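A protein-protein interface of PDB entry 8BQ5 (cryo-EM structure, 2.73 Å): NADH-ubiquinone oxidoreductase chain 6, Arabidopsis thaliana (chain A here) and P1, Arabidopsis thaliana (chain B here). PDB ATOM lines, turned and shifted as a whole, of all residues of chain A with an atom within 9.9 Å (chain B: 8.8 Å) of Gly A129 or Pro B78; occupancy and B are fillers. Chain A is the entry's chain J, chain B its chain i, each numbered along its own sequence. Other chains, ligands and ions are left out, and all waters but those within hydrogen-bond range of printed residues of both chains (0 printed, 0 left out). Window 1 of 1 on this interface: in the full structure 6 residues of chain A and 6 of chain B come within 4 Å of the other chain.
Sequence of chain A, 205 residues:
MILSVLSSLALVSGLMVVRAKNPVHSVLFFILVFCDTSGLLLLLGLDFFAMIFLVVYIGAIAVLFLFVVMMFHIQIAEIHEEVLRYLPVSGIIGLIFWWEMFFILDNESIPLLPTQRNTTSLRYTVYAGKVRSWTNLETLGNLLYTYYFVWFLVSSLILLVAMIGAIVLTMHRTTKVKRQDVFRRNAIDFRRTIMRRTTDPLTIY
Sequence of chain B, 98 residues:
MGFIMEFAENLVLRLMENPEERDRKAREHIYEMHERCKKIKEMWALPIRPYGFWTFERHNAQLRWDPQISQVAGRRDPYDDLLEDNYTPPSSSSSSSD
The side-chain carboxylate (OD1) of Asp B77 sits at hydrogen-bond distance from the backbone NH (N) of Tyr B79 (3.0 Å).
CG1 of Val A126 touches OH of Tyr B79, 3.8 Å away.
CB of Ala A128 touches CB of Pro B78 (3.7 Å).
Ala A128 touches Tyr B79 (CB to CE1, 3.8 Å).
CB of Ala A128 touches CD2 of Leu B82, 3.6 Å away.
Gly A129 touches Pro B78 (N to CB, 3.7 Å).
Printed residues of chain B within 4 Å of Val A126: Tyr B79.
Ala A128 touches just these residues of chain B: Pro B78, Tyr B79 and Leu B82.
Gly A129 touches just one residue of chain B: Pro B78.
Of the printed residues of chain A, Pro B78 touches Ala A128 (3.7 Å) and Gly A129 (3.7 Å).
Of the printed residues of chain A, Tyr B79 touches Val A126 (3.8 Å) and Ala A128 (3.8 Å).
Of the printed residues of chain A, Leu B82 touches Ala A128 (3.6 Å).
The nearest residue of chain B that does not touch Gly A129 is Leu B82 (6.0 Å).
The nearest printed residue of chain A that does not touch Tyr B79 is Tyr A127 (5.6 Å).
Hydrophobic or aromatic side chains of chain A within 4 Å of the printed part of chain B: Val A126 and Ala A128.
Of the 10 printed residues of chain B, 3 touch a printed residue of chain A.
Hydrophobic or aromatic side chains of chain B that line the printed part of chain A: Pro B78, Tyr B79 and Leu B82.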
ATOM      1  N   THR A 125     -14.760 -35.124  23.865  1.00  0.00           N
ATOM      2  CA  THR A 125     -14.135 -33.771  23.851  1.00  0.00           C
ATOM      3  C   THR A 125     -12.689 -33.832  24.351  1.00  0.00           C
ATOM      4  O   THR A 125     -12.460 -34.328  25.462  1.00  0.00           O
ATOM      5  CB  THR A 125     -14.969 -32.779  24.666  1.00  0.00           C
ATOM      6  OG1 THR A 125     -16.221 -32.617  24.000  1.00  0.00           O
ATOM      7  CG2 THR A 125     -14.309 -31.429  24.841  1.00  0.00           C
ATOM      8  N   VAL A 126     -11.750 -33.339  23.546  1.00  0.00           N
ATOM      9  CA  VAL A 126     -10.339 -33.336  23.911  1.00  0.00           C
ATOM     10  C   VAL A 126      -9.957 -31.901  24.243  1.00  0.00           C
ATOM     11  O   VAL A 126     -10.025 -31.015  23.382  1.00  0.00           O
ATOM     12  CB  VAL A 126      -9.460 -33.900  22.787  1.00  0.00           C
ATOM     13  CG1 VAL A 126      -8.022 -34.037  23.256  1.00  0.00           C
ATOM     14  CG2 VAL A 126     -10.005 -35.237  22.324  1.00  0.00           C
ATOM     15  N   TYR A 127      -9.550 -31.664  25.489  1.00  0.00           N
ATOM     16  CA  TYR A 127      -9.207 -30.315  25.911  1.00  0.00           C
ATOM     17  C   TYR A 127      -7.786 -29.920  25.538  1.00  0.00           C
ATOM     18  O   TYR A 127      -7.434 -28.743  25.666  1.00  0.00           O
ATOM     19  CB  TYR A 127      -9.391 -30.167  27.422  1.00  0.00           C
ATOM     20  CG  TYR A 127     -10.828 -30.277  27.862  1.00  0.00           C
ATOM     21  CD1 TYR A 127     -11.666 -29.174  27.833  1.00  0.00           C
ATOM     22  CD2 TYR A 127     -11.346 -31.483  28.307  1.00  0.00           C
ATOM     23  CE1 TYR A 127     -12.978 -29.269  28.231  1.00  0.00           C
ATOM     24  CE2 TYR A 127     -12.658 -31.589  28.710  1.00  0.00           C
ATOM     25  CZ  TYR A 127     -13.469 -30.478  28.670  1.00  0.00           C
ATOM     26  OH  TYR A 127     -14.779 -30.572  29.068  1.00  0.00           O
ATOM     27  N   ALA A 128      -6.964 -30.870  25.090  1.00  0.00           N
ATOM     28  CA  ALA A 128      -5.569 -30.558  24.797  1.00  0.00           C
ATOM     29  C   ALA A 128      -5.449 -29.604  23.614  1.00  0.00           C
ATOM     30  O   ALA A 128      -4.641 -28.669  23.642  1.00  0.00           O
ATOM     31  CB  ALA A 128      -4.788 -31.844  24.541  1.00  0.00           C
ATOM     32  N   GLY A 129      -6.246 -29.819  22.572  1.00  0.00           N
ATOM     33  CA  GLY A 129      -6.224 -28.933  21.425  1.00  0.00           C
ATOM     34  C   GLY A 129      -6.976 -27.635  21.607  1.00  0.00           C
ATOM     35  O   GLY A 129      -6.960 -26.797  20.702  1.00  0.00           O
ATOM     36  N   LYS A 130      -7.633 -27.444  22.748  1.00  0.00           N
ATOM     37  CA  LYS A 130      -8.398 -26.238  23.023  1.00  0.00           C
ATOM     38  C   LYS A 130      -7.677 -25.273  23.952  1.00  0.00           C
ATOM     39  O   LYS A 130      -8.240 -24.230  24.293  1.00  0.00           O
ATOM     40  CB  LYS A 130      -9.754 -26.603  23.628  1.00  0.00           C
ATOM     41  CG  LYS A 130     -10.786 -27.061  22.624  1.00  0.00           C
ATOM     42  CD  LYS A 130     -11.997 -27.636  23.334  1.00  0.00           C
ATOM     43  CE  LYS A 130     -12.806 -28.526  22.412  1.00  0.00           C
ATOM     44  NZ  LYS A 130     -14.081 -27.881  22.002  1.00  0.00           N
ATOM     45  N   VAL A 131      -6.459 -25.600  24.384  1.00  0.00           N
ATOM     46  CA  VAL A 131      -5.743 -24.728  25.309  1.00  0.00           C
ATOM     47  C   VAL A 131      -5.349 -23.431  24.619  1.00  0.00           C
ATOM     48  O   VAL A 131      -5.550 -22.335  25.157  1.00  0.00           O
ATOM     49  CB  VAL A 131      -4.518 -25.459  25.883  1.00  0.00           C
ATOM     50  CG1 VAL A 131      -3.681 -24.514  26.724  1.00  0.00           C
ATOM     51  CG2 VAL A 131      -4.955 -26.666  26.686  1.00  0.00           C
ATOM     52  N   ARG A 132      -4.777 -23.534  23.420  1.00  0.00           N
ATOM     53  CA  ARG A 132      -4.425 -22.384  22.586  1.00  0.00           C
ATOM     54  C   ARG A 132      -5.006 -22.663  21.203  1.00  0.00           C
ATOM     55  O   ARG A 132      -4.518 -23.533  20.477  1.00  0.00           O
ATOM     56  CB  ARG A 132      -2.920 -22.163  22.532  1.00  0.00           C
ATOM     57  CG  ARG A 132      -2.503 -21.051  21.585  1.00  0.00           C
ATOM     58  CD  ARG A 132      -1.000 -20.839  21.600  1.00  0.00           C
ATOM     59  NE  ARG A 132      -0.595 -19.762  20.705  1.00  0.00           N
ATOM     60  CZ  ARG A 132       0.605 -19.201  20.702  1.00  0.00           C
ATOM     61  NH1 ARG A 132       1.548 -19.580  21.549  1.00  0.00           N
ATOM     62  NH2 ARG A 132       0.867 -18.234  19.827  1.00  0.00           N
ATOM     63  N   SER A 133      -6.047 -21.922  20.845  1.00  0.00           N
ATOM     64  CA  SER A 133      -6.704 -22.121  19.564  1.00  0.00           C
ATOM     65  C   SER A 133      -6.104 -21.215  18.496  1.00  0.00           C
ATOM     66  O   SER A 133      -5.806 -20.045  18.747  1.00  0.00           O
ATOM     67  CB  SER A 133      -8.203 -21.858  19.695  1.00  0.00           C
ATOM     68  OG  SER A 133      -8.452 -20.718  20.499  1.00  0.00           O
ATOM     69  N   TRP A 134      -5.918 -21.774  17.304  1.00  0.00           N
ATOM     70  CA  TRP A 134      -5.471 -21.027  16.138  1.00  0.00           C
ATOM     71  C   TRP A 134      -6.680 -20.600  15.320  1.00  0.00           C
ATOM     72  O   TRP A 134      -7.604 -21.389  15.106  1.00  0.00           O
ATOM     73  CB  TRP A 134      -4.543 -21.872  15.261  1.00  0.00           C
ATOM     74  CG  TRP A 134      -3.113 -21.926  15.706  1.00  0.00           C
ATOM     75  CD1 TRP A 134      -2.633 -21.683  16.958  1.00  0.00           C
ATOM     76  CD2 TRP A 134      -1.979 -22.273  14.901  1.00  0.00           C
ATOM     77  NE1 TRP A 134      -1.269 -21.845  16.981  1.00  0.00           N
ATOM     78  CE2 TRP A 134      -0.843 -22.209  15.730  1.00  0.00           C
ATOM     79  CE3 TRP A 134      -1.812 -22.626  13.557  1.00  0.00           C
ATOM     80  CZ2 TRP A 134       0.440 -22.485  15.263  1.00  0.00           C
ATOM     81  CZ3 TRP A 134      -0.538 -22.901  13.096  1.00  0.00           C
ATOM     82  CH2 TRP A 134       0.570 -22.828  13.946  1.00  0.00           C
ATOM     83  N   THR A 135      -6.675 -19.354  14.860  1.00  0.00           N
ATOM     84  CA  THR A 135      -7.690 -18.951  13.905  1.00  0.00           C
ATOM     85  C   THR A 135      -7.351 -19.510  12.526  1.00  0.00           C
ATOM     86  O   THR A 135      -6.229 -19.948  12.261  1.00  0.00           O
ATOM     87  CB  THR A 135      -7.819 -17.428  13.847  1.00  0.00           C
ATOM     88  OG1 THR A 135      -6.704 -16.871  13.143  1.00  0.00           O
ATOM     89  CG2 THR A 135      -7.872 -16.843  15.247  1.00  0.00           C
ATOM     90  N   ARG B  75       1.526 -28.890  13.140  1.00  0.00           N
ATOM     91  CA  ARG B  75       1.360 -30.292  12.778  1.00  0.00           C
ATOM     92  C   ARG B  75       1.700 -31.231  13.931  1.00  0.00           C
ATOM     93  O   ARG B  75       2.061 -32.389  13.690  1.00  0.00           O
ATOM     94  CB  ARG B  75       2.214 -30.645  11.558  1.00  0.00           C
ATOM     95  CG  ARG B  75       3.708 -30.501  11.779  1.00  0.00           C
ATOM     96  CD  ARG B  75       4.447 -30.578  10.463  1.00  0.00           C
ATOM     97  NE  ARG B  75       4.439 -31.930   9.919  1.00  0.00           N
ATOM     98  CZ  ARG B  75       3.714 -32.311   8.878  1.00  0.00           C
ATOM     99  NH1 ARG B  75       2.903 -31.470   8.257  1.00  0.00           N
ATOM    100  NH2 ARG B  75       3.803 -33.566   8.451  1.00  0.00           N
ATOM    101  N   ARG B  76       1.588 -30.771  15.170  1.00  0.00           N
ATOM    102  CA  ARG B  76       1.918 -31.586  16.326  1.00  0.00           C
ATOM    103  C   ARG B  76       0.666 -32.193  16.944  1.00  0.00           C
ATOM    104  O   ARG B  76      -0.424 -31.617  16.890  1.00  0.00           O
ATOM    105  CB  ARG B  76       2.655 -30.757  17.374  1.00  0.00           C
ATOM    106  CG  ARG B  76       3.810 -29.958  16.827  1.00  0.00           C
ATOM    107  CD  ARG B  76       4.659 -29.394  17.945  1.00  0.00           C
ATOM    108  NE  ARG B  76       5.355 -30.447  18.673  1.00  0.00           N
ATOM    109  CZ  ARG B  76       5.975 -30.273  19.831  1.00  0.00           C
ATOM    110  NH1 ARG B  76       6.019 -29.090  20.421  1.00  0.00           N
ATOM    111  NH2 ARG B  76       6.572 -31.312  20.409  1.00  0.00           N
ATOM    112  N   ASP B  77       0.834 -33.375  17.521  1.00  0.00           N
ATOM    113  CA  ASP B  77      -0.190 -33.938  18.386  1.00  0.00           C
ATOM    114  C   ASP B  77      -0.349 -33.017  19.592  1.00  0.00           C
ATOM    115  O   ASP B  77       0.657 -32.588  20.171  1.00  0.00           O
ATOM    116  CB  ASP B  77       0.216 -35.360  18.797  1.00  0.00           C
ATOM    117  CG  ASP B  77      -0.346 -35.799  20.151  1.00  0.00           C
ATOM    118  OD1 ASP B  77      -1.463 -35.401  20.536  1.00  0.00           O
ATOM    119  OD2 ASP B  77       0.351 -36.572  20.840  1.00  0.00           O
ATOM    120  N   PRO B  78      -1.577 -32.670  19.985  1.00  0.00           N
ATOM    121  CA  PRO B  78      -1.742 -31.685  21.065  1.00  0.00           C
ATOM    122  C   PRO B  78      -1.072 -32.070  22.369  1.00  0.00           C
ATOM    123  O   PRO B  78      -0.705 -31.169  23.129  1.00  0.00           O
ATOM    124  CB  PRO B  78      -3.268 -31.581  21.216  1.00  0.00           C
ATOM    125  CG  PRO B  78      -3.833 -32.737  20.430  1.00  0.00           C
ATOM    126  CD  PRO B  78      -2.857 -32.973  19.332  1.00  0.00           C
ATOM    127  N   TYR B  79      -0.863 -33.362  22.639  1.00  0.00           N
ATOM    128  CA  TYR B  79      -0.313 -33.773  23.929  1.00  0.00           C
ATOM    129  C   TYR B  79       1.182 -33.497  24.069  1.00  0.00           C
ATOM    130  O   TYR B  79       1.663 -33.378  25.201  1.00  0.00           O
ATOM    131  CB  TYR B  79      -0.621 -35.247  24.186  1.00  0.00           C
ATOM    132  CG  TYR B  79      -2.048 -35.456  24.633  1.00  0.00           C
ATOM    133  CD1 TYR B  79      -2.494 -34.963  25.853  1.00  0.00           C
ATOM    134  CD2 TYR B  79      -2.960 -36.109  23.819  1.00  0.00           C
ATOM    135  CE1 TYR B  79      -3.800 -35.139  26.257  1.00  0.00           C
ATOM    136  CE2 TYR B  79      -4.266 -36.289  24.213  1.00  0.00           C
ATOM    137  CZ  TYR B  79      -4.681 -35.803  25.432  1.00  0.00           C
ATOM    138  OH  TYR B  79      -5.986 -35.981  25.826  1.00  0.00           O
ATOM    139  N   ASP B  80       1.928 -33.381  22.967  1.00  0.00           N
ATOM    140  CA  ASP B  80       3.350 -33.062  23.096  1.00  0.00           C
ATOM    141  C   ASP B  80       3.566 -31.671  23.675  1.00  0.00           C
ATOM    142  O   ASP B  80       4.584 -31.428  24.328  1.00  0.00           O
ATOM    143  CB  ASP B  80       4.074 -33.187  21.754  1.00  0.00           C
ATOM    144  CG  ASP B  80       4.222 -34.618  21.299  1.00  0.00           C
ATOM    145  OD1 ASP B  80       4.030 -35.521  22.127  1.00  0.00           O
ATOM    146  OD2 ASP B  80       4.534 -34.842  20.109  1.00  0.00           O
ATOM    147  N   ASP B  81       2.633 -30.747  23.444  1.00  0.00           N
ATOM    148  CA  ASP B  81       2.725 -29.446  24.099  1.00  0.00           C
ATOM    149  C   ASP B  81       2.522 -29.572  25.605  1.00  0.00           C
ATOM    150  O   ASP B  81       3.102 -28.804  26.381  1.00  0.00           O
ATOM    151  CB  ASP B  81       1.712 -28.472  23.498  1.00  0.00           C
ATOM    152  CG  ASP B  81       1.566 -28.632  22.001  1.00  0.00           C
ATOM    153  OD1 ASP B  81       2.591 -28.857  21.326  1.00  0.00           O
ATOM    154  OD2 ASP B  81       0.429 -28.527  21.494  1.00  0.00           O
ATOM    155  N   LEU B  82       1.697 -30.529  26.036  1.00  0.00           N
ATOM    156  CA  LEU B  82       1.436 -30.688  27.463  1.00  0.00           C
ATOM    157  C   LEU B  82       2.634 -31.257  28.210  1.00  0.00           C
ATOM    158  O   LEU B  82       2.851 -30.909  29.376  1.00  0.00           O
ATOM    159  CB  LEU B  82       0.209 -31.574  27.693  1.00  0.00           C
ATOM    160  CG  LEU B  82      -1.157 -31.028  27.276  1.00  0.00           C
ATOM    161  CD1 LEU B  82      -1.225 -29.530  27.488  1.00  0.00           C
ATOM    162  CD2 LEU B  82      -1.500 -31.355  25.883  1.00  0.00           C
ATOM    163  N   LEU B  83       3.415 -32.130  27.577  1.00  0.00           N
ATOM    164  CA  LEU B  83       4.543 -32.761  28.248  1.00  0.00           C
ATOM    165  C   LEU B  83       5.900 -32.237  27.801  1.00  0.00           C
ATOM    166  O   LEU B  83       6.920 -32.839  28.155  1.00  0.00           O
ATOM    167  CB  LEU B  83       4.508 -34.279  28.052  1.00  0.00           C
ATOM    168  CG  LEU B  83       3.277 -34.996  28.598  1.00  0.00           C
ATOM    169  CD1 LEU B  83       2.877 -36.132  27.684  1.00  0.00           C
ATOM    170  CD2 LEU B  83       3.551 -35.501  30.002  1.00  0.00           C
ATOM    171  N   GLU B  84       5.948 -31.149  27.043  1.00  0.00           N
ATOM    172  CA  GLU B  84       7.233 -30.565  26.683  1.00  0.00           C
ATOM    173  C   GLU B  84       7.298 -29.097  27.073  1.00  0.00           C
ATOM    174  O   GLU B  84       8.111 -28.711  27.912  1.00  0.00           O
ATOM    175  CB  GLU B  84       7.508 -30.728  25.190  1.00  0.00           C
ATOM    176  CG  GLU B  84       8.249 -32.004  24.851  1.00  0.00           C
ATOM    177  CD  GLU B  84       9.697 -31.956  25.290  1.00  0.00           C
ATOM    178  OE1 GLU B  84      10.291 -30.859  25.254  1.00  0.00           O
ATOM    179  OE2 GLU B  84      10.241 -33.013  25.671  1.00  0.00           O
